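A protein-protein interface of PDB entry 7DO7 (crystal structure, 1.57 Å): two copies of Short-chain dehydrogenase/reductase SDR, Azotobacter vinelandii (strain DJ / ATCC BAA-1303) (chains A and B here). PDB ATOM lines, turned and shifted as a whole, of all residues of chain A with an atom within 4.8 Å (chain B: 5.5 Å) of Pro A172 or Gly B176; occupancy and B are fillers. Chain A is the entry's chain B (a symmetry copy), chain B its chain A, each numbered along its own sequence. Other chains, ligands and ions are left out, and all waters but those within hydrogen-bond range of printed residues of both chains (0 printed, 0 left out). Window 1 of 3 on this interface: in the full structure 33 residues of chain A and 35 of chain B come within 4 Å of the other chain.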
ATOM      1  N   GLN A 167      -5.381  27.734   1.593  1.00  0.00           N
ATOM      2  CA  GLN A 167      -5.873  26.429   1.182  1.00  0.00           C
ATOM      3  C   GLN A 167      -6.159  25.535   2.383  1.00  0.00           C
ATOM      4  O   GLN A 167      -6.103  24.304   2.264  1.00  0.00           O
ATOM      5  CB  GLN A 167      -4.878  25.722   0.257  1.00  0.00           C
ATOM      6  CG  GLN A 167      -4.596  26.468  -1.057  1.00  0.00           C
ATOM      7  CD  GLN A 167      -3.355  25.942  -1.765  1.00  0.00           C
ATOM      8  OE1 GLN A 167      -2.239  26.078  -1.262  1.00  0.00           O
ATOM      9  NE2 GLN A 167      -3.543  25.329  -2.926  1.00  0.00           N
ATOM     10  N   THR A 168      -6.481  26.119   3.544  1.00  0.00           N
ATOM     11  CA  THR A 168      -6.759  25.276   4.712  1.00  0.00           C
ATOM     12  C   THR A 168      -7.945  24.352   4.475  1.00  0.00           C
ATOM     13  O   THR A 168      -8.026  23.276   5.083  1.00  0.00           O
ATOM     14  CB  THR A 168      -7.034  26.119   5.957  1.00  0.00           C
ATOM     15  OG1 THR A 168      -8.095  27.044   5.686  1.00  0.00           O
ATOM     16  CG2 THR A 168      -5.802  26.888   6.385  1.00  0.00           C
ATOM     17  N   HIS A 169      -8.891  24.771   3.636  1.00  0.00           N
ATOM     18  CA  HIS A 169     -10.016  23.925   3.253  1.00  0.00           C
ATOM     19  C   HIS A 169      -9.661  22.916   2.175  1.00  0.00           C
ATOM     20  O   HIS A 169     -10.378  21.924   2.007  1.00  0.00           O
ATOM     21  CB  HIS A 169     -11.181  24.784   2.746  1.00  0.00           C
ATOM     22  CG  HIS A 169     -10.816  25.704   1.617  1.00  0.00           C
ATOM     23  ND1 HIS A 169      -9.658  26.452   1.603  1.00  0.00           N
ATOM     24  CD2 HIS A 169     -11.471  26.009   0.469  1.00  0.00           C
ATOM     25  CE1 HIS A 169      -9.608  27.168   0.492  1.00  0.00           C
ATOM     26  NE2 HIS A 169     -10.700  26.923  -0.211  1.00  0.00           N
ATOM     27  N   TYR A 170      -8.589  23.156   1.427  1.00  0.00           N
ATOM     28  CA  TYR A 170      -8.251  22.375   0.248  1.00  0.00           C
ATOM     29  C   TYR A 170      -7.209  21.306   0.528  1.00  0.00           C
ATOM     30  O   TYR A 170      -7.383  20.156   0.107  1.00  0.00           O
ATOM     31  CB  TYR A 170      -7.744  23.329  -0.834  1.00  0.00           C
ATOM     32  CG  TYR A 170      -7.107  22.715  -2.057  1.00  0.00           C
ATOM     33  CD1 TYR A 170      -7.886  22.231  -3.105  1.00  0.00           C
ATOM     34  CD2 TYR A 170      -5.723  22.686  -2.193  1.00  0.00           C
ATOM     35  CE1 TYR A 170      -7.303  21.696  -4.243  1.00  0.00           C
ATOM     36  CE2 TYR A 170      -5.132  22.157  -3.321  1.00  0.00           C
ATOM     37  CZ  TYR A 170      -5.925  21.670  -4.348  1.00  0.00           C
ATOM     38  OH  TYR A 170      -5.348  21.148  -5.477  1.00  0.00           O
ATOM     39  N   THR A 171      -6.121  21.653   1.223  1.00  0.00           N
ATOM     40  CA  THR A 171      -5.087  20.647   1.451  1.00  0.00           C
ATOM     41  C   THR A 171      -5.625  19.421   2.176  1.00  0.00           C
ATOM     42  O   THR A 171      -5.211  18.305   1.814  1.00  0.00           O
ATOM     43  CB  THR A 171      -3.852  21.239   2.169  1.00  0.00           C
ATOM     44  OG1 THR A 171      -4.117  21.532   3.556  1.00  0.00           O
ATOM     45  CG2 THR A 171      -3.363  22.495   1.466  1.00  0.00           C
ATOM     46  N   PRO A 172      -6.564  19.518   3.125  1.00  0.00           N
ATOM     47  CA  PRO A 172      -7.085  18.274   3.720  1.00  0.00           C
ATOM     48  C   PRO A 172      -7.782  17.379   2.724  1.00  0.00           C
ATOM     49  O   PRO A 172      -7.795  16.151   2.914  1.00  0.00           O
ATOM     50  CB  PRO A 172      -8.046  18.778   4.808  1.00  0.00           C
ATOM     51  CG  PRO A 172      -7.495  20.130   5.177  1.00  0.00           C
ATOM     52  CD  PRO A 172      -7.077  20.699   3.847  1.00  0.00           C
ATOM     53  N   THR A 173      -8.383  17.934   1.668  1.00  0.00           N
ATOM     54  CA  THR A 173      -8.986  17.047   0.682  1.00  0.00           C
ATOM     55  C   THR A 173      -7.925  16.339  -0.148  1.00  0.00           C
ATOM     56  O   THR A 173      -8.126  15.190  -0.553  1.00  0.00           O
ATOM     57  CB  THR A 173      -9.964  17.799  -0.235  1.00  0.00           C
ATOM     58  OG1 THR A 173      -9.260  18.695  -1.118  1.00  0.00           O
ATOM     59  CG2 THR A 173     -10.982  18.595   0.585  1.00  0.00           C
ATOM     60  N   LYS A 174      -6.795  17.000  -0.425  1.00  0.00           N
ATOM     61  CA  LYS A 174      -5.744  16.337  -1.189  1.00  0.00           C
ATOM     62  C   LYS A 174      -5.033  15.286  -0.341  1.00  0.00           C
ATOM     63  O   LYS A 174      -4.751  14.177  -0.820  1.00  0.00           O
ATOM     64  CB  LYS A 174      -4.754  17.375  -1.728  1.00  0.00           C
ATOM     65  CG  LYS A 174      -5.403  18.494  -2.566  1.00  0.00           C
ATOM     66  CD  LYS A 174      -5.694  18.039  -3.998  1.00  0.00           C
ATOM     67  CE  LYS A 174      -7.180  17.870  -4.229  1.00  0.00           C
ATOM     68  NZ  LYS A 174      -7.480  17.396  -5.617  1.00  0.00           N
ATOM     69  N   ALA A 175      -4.758  15.605   0.927  1.00  0.00           N
ATOM     70  CA  ALA A 175      -4.235  14.581   1.834  1.00  0.00           C
ATOM     71  C   ALA A 175      -5.238  13.451   2.006  1.00  0.00           C
ATOM     72  O   ALA A 175      -4.858  12.269   2.038  1.00  0.00           O
ATOM     73  CB  ALA A 175      -3.897  15.201   3.190  1.00  0.00           C
ATOM     74  N   GLY A 176      -6.525  13.796   2.102  1.00  0.00           N
ATOM     75  CA  GLY A 176      -7.550  12.771   2.225  1.00  0.00           C
ATOM     76  C   GLY A 176      -7.581  11.824   1.040  1.00  0.00           C
ATOM     77  O   GLY A 176      -7.715  10.611   1.208  1.00  0.00           O
ATOM     78  N   LEU B 129     -13.298  15.669  10.824  1.00  0.00           N
ATOM     79  CA  LEU B 129     -12.574  16.673  10.049  1.00  0.00           C
ATOM     80  C   LEU B 129     -13.330  17.991   9.968  1.00  0.00           C
ATOM     81  O   LEU B 129     -12.771  19.038  10.333  1.00  0.00           O
ATOM     82  CB  LEU B 129     -12.293  16.126   8.644  1.00  0.00           C
ATOM     83  CG  LEU B 129     -11.518  17.069   7.727  1.00  0.00           C
ATOM     84  CD1 LEU B 129     -10.167  17.376   8.352  1.00  0.00           C
ATOM     85  CD2 LEU B 129     -11.359  16.460   6.330  1.00  0.00           C
ATOM     86  N   THR B 171      -9.392   6.990   7.618  1.00  0.00           N
ATOM     87  CA  THR B 171      -8.020   7.456   7.429  1.00  0.00           C
ATOM     88  C   THR B 171      -7.962   8.785   6.677  1.00  0.00           C
ATOM     89  O   THR B 171      -7.115   9.616   7.043  1.00  0.00           O
ATOM     90  CB  THR B 171      -7.120   6.388   6.772  1.00  0.00           C
ATOM     91  OG1 THR B 171      -7.431   6.206   5.380  1.00  0.00           O
ATOM     92  CG2 THR B 171      -7.223   5.057   7.507  1.00  0.00           C
ATOM     93  N   PRO B 172      -8.840   9.091   5.705  1.00  0.00           N
ATOM     94  CA  PRO B 172      -8.792  10.436   5.102  1.00  0.00           C
ATOM     95  C   PRO B 172      -9.067  11.568   6.080  1.00  0.00           C
ATOM     96  O   PRO B 172      -8.562  12.680   5.875  1.00  0.00           O
ATOM     97  CB  PRO B 172      -9.872  10.375   4.011  1.00  0.00           C
ATOM     98  CG  PRO B 172      -9.947   8.939   3.657  1.00  0.00           C
ATOM     99  CD  PRO B 172      -9.769   8.213   4.966  1.00  0.00           C
ATOM    100  N   THR B 173      -9.864  11.331   7.129  1.00  0.00           N
ATOM    101  CA  THR B 173     -10.102  12.371   8.119  1.00  0.00           C
ATOM    102  C   THR B 173      -8.875  12.587   8.997  1.00  0.00           C
ATOM    103  O   THR B 173      -8.603  13.718   9.417  1.00  0.00           O
ATOM    104  CB  THR B 173     -11.333  12.036   8.990  1.00  0.00           C
ATOM    105  OG1 THR B 173     -11.014  11.034   9.960  1.00  0.00           O
ATOM    106  CG2 THR B 173     -12.524  11.573   8.154  1.00  0.00           C
ATOM    107  N   LYS B 174      -8.124  11.514   9.286  1.00  0.00           N
ATOM    108  CA  LYS B 174      -6.914  11.663  10.086  1.00  0.00           C
ATOM    109  C   LYS B 174      -5.800  12.311   9.281  1.00  0.00           C
ATOM    110  O   LYS B 174      -5.056  13.149   9.802  1.00  0.00           O
ATOM    111  CB  LYS B 174      -6.460  10.305  10.612  1.00  0.00           C
ATOM    112  CG  LYS B 174      -7.480   9.658  11.506  1.00  0.00           C
ATOM    113  CD  LYS B 174      -7.511  10.332  12.869  1.00  0.00           C
ATOM    114  CE  LYS B 174      -8.823  11.047  13.103  1.00  0.00           C
ATOM    115  NZ  LYS B 174      -8.993  11.506  14.517  1.00  0.00           N
ATOM    116  N   ALA B 175      -5.669  11.926   8.011  1.00  0.00           N
ATOM    117  CA  ALA B 175      -4.713  12.602   7.145  1.00  0.00           C
ATOM    118  C   ALA B 175      -5.130  14.047   6.911  1.00  0.00           C
ATOM    119  O   ALA B 175      -4.281  14.948   6.890  1.00  0.00           O
ATOM    120  CB  ALA B 175      -4.580  11.851   5.823  1.00  0.00           C
ATOM    121  N   GLY B 176      -6.439  14.287   6.759  1.00  0.00           N
ATOM    122  CA  GLY B 176      -6.910  15.653   6.584  1.00  0.00           C
ATOM    123  C   GLY B 176      -6.607  16.527   7.787  1.00  0.00           C
ATOM    124  O   GLY B 176      -6.290  17.712   7.639  1.00  0.00           O
ATOM    125  N   LEU B 177      -6.719  15.956   9.000  1.00  0.00           N
ATOM    126  CA  LEU B 177      -6.415  16.710  10.218  1.00  0.00           C
ATOM    127  C   LEU B 177      -4.955  17.119  10.266  1.00  0.00           C
ATOM    128  O   LEU B 177      -4.630  18.248  10.650  1.00  0.00           O
ATOM    129  CB  LEU B 177      -6.751  15.878  11.449  1.00  0.00           C
ATOM    130  CG  LEU B 177      -8.179  15.928  11.951  1.00  0.00           C
ATOM    131  CD1 LEU B 177      -8.280  14.868  13.054  1.00  0.00           C
ATOM    132  CD2 LEU B 177      -8.496  17.318  12.475  1.00  0.00           C
ATOM    133  N   LEU B 178      -4.058  16.198   9.906  1.00  0.00           N
ATOM    134  CA  LEU B 178      -2.638  16.510   9.846  1.00  0.00           C
ATOM    135  C   LEU B 178      -2.387  17.632   8.854  1.00  0.00           C
ATOM    136  O   LEU B 178      -1.677  18.600   9.152  1.00  0.00           O
ATOM    137  CB  LEU B 178      -1.855  15.255   9.446  1.00  0.00           C
ATOM    138  CG  LEU B 178      -0.329  15.211   9.545  1.00  0.00           C
ATOM    139  CD1 LEU B 178       0.139  13.762   9.554  1.00  0.00           C
ATOM    140  CD2 LEU B 178       0.364  15.968   8.416  1.00  0.00           C
ATOM    141  N   SER B 179      -2.991  17.527   7.676  1.00  0.00           N
ATOM    142  CA  SER B 179      -2.805  18.540   6.649  1.00  0.00           C
ATOM    143  C   SER B 179      -3.396  19.877   7.076  1.00  0.00           C
ATOM    144  O   SER B 179      -2.821  20.940   6.795  1.00  0.00           O
ATOM    145  CB  SER B 179      -3.434  18.056   5.345  1.00  0.00           C
ATOM    146  OG  SER B 179      -3.381  19.092   4.395  1.00  0.00           O
ATOM    147  N   LEU B 180      -4.542  19.844   7.761  1.00  0.00           N
ATOM    148  CA  LEU B 180      -5.097  21.066   8.330  1.00  0.00           C
ATOM    149  C   LEU B 180      -4.107  21.738   9.284  1.00  0.00           C
ATOM    150  O   LEU B 180      -3.954  22.965   9.270  1.00  0.00           O
ATOM    151  CB  LEU B 180      -6.413  20.753   9.047  1.00  0.00           C
ATOM    152  CG  LEU B 180      -7.051  21.984   9.689  1.00  0.00           C
ATOM    153  CD1 LEU B 180      -7.379  23.048   8.626  1.00  0.00           C
ATOM    154  CD2 LEU B 180      -8.285  21.575  10.483  1.00  0.00           C
ATOM    155  N   MET B 181      -3.423  20.956  10.124  1.00  0.00           N
ATOM    156  CA  MET B 181      -2.424  21.569  10.997  1.00  0.00           C
ATOM    157  C   MET B 181      -1.285  22.192  10.198  1.00  0.00           C
ATOM    158  O   MET B 181      -0.813  23.279  10.531  1.00  0.00           O
ATOM    159  CB  MET B 181      -1.897  20.546  12.003  1.00  0.00           C
ATOM    160  CG  MET B 181      -2.934  20.126  13.025  1.00  0.00           C
ATOM    161  SD  MET B 181      -3.595  21.472  14.057  1.00  0.00           S
ATOM    162  CE  MET B 181      -5.078  21.995  13.167  1.00  0.00           C
ATOM    163  N   SER B 183      -1.391  23.502   7.142  1.00  0.00           N
ATOM    164  CA  SER B 183      -1.847  24.730   6.491  1.00  0.00           C
ATOM    165  C   SER B 183      -2.156  25.823   7.507  1.00  0.00           C
ATOM    166  O   SER B 183      -1.857  26.998   7.271  1.00  0.00           O
ATOM    167  CB  SER B 183      -3.067  24.427   5.625  1.00  0.00           C
ATOM    168  OG  SER B 183      -2.678  23.662   4.495  1.00  0.00           O
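OG of Ser B183 lies within hydrogen-bond range of OG1 of Thr A171 (2.7 Å).
N of Pro A172 sits close to OG of Ser B179 (3.5 Å).
The side-chain hydroxyl (OG) of Ser B179 is in hydrogen-bond range of the side-chain hydroxyl (OG1) of Thr A171, 2.7 Å away.
Among the printed residues, pairs that only touch across the chains: Pro A172 with Gly B176 (3.5 Å), Gly A176 with Pro B172 (3.5 Å), Ala A175 with Ser B179 (3.6 Å), Thr A168 with Leu B180 (3.6 Å), Ala A175 with Ala B175 (3.7 Å), Thr A168 with Ser B183 (3.8 Å) and Pro A172 with Leu B180 (3.9 Å).
Pro A172 touches just these residues of chain B: Gly B176, Ser B179 and Leu B180.
Gly B176 touches just one residue of chain A: Pro A172.
Of the printed residues of chain A, Ser B179 touches Thr A171 (2.7 Å), Pro A172 (3.5 Å) and Ala A175 (3.6 Å).
Printed residues of chain A within 4 Å of Leu B180: Thr A168 (3.6 Å) and Pro A172 (3.9 Å).
The nearest residue of chain B that does not touch Pro A172 is Leu B129 (4.3 Å).
The nearest residue of chain A that does not touch Gly B176 is Ala A175 (4.5 Å).
Hydrophobic or aromatic side chains of chain B within 4 Å of the printed part of chain A: Pro B172, Ala B175 and Leu B180.
Printed residues of chain A that touch a printed residue of chain B: Thr A168, Thr A171, Pro A172, Ala A175 and Gly A176.
Among the printed residues, 10 pairs touch across the chains.
Pro A172 touches Gly B176, and with the chains exchanged Gly A176 touches Pro B172.
Ala B175 touches its own counterpart, Ala A175.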
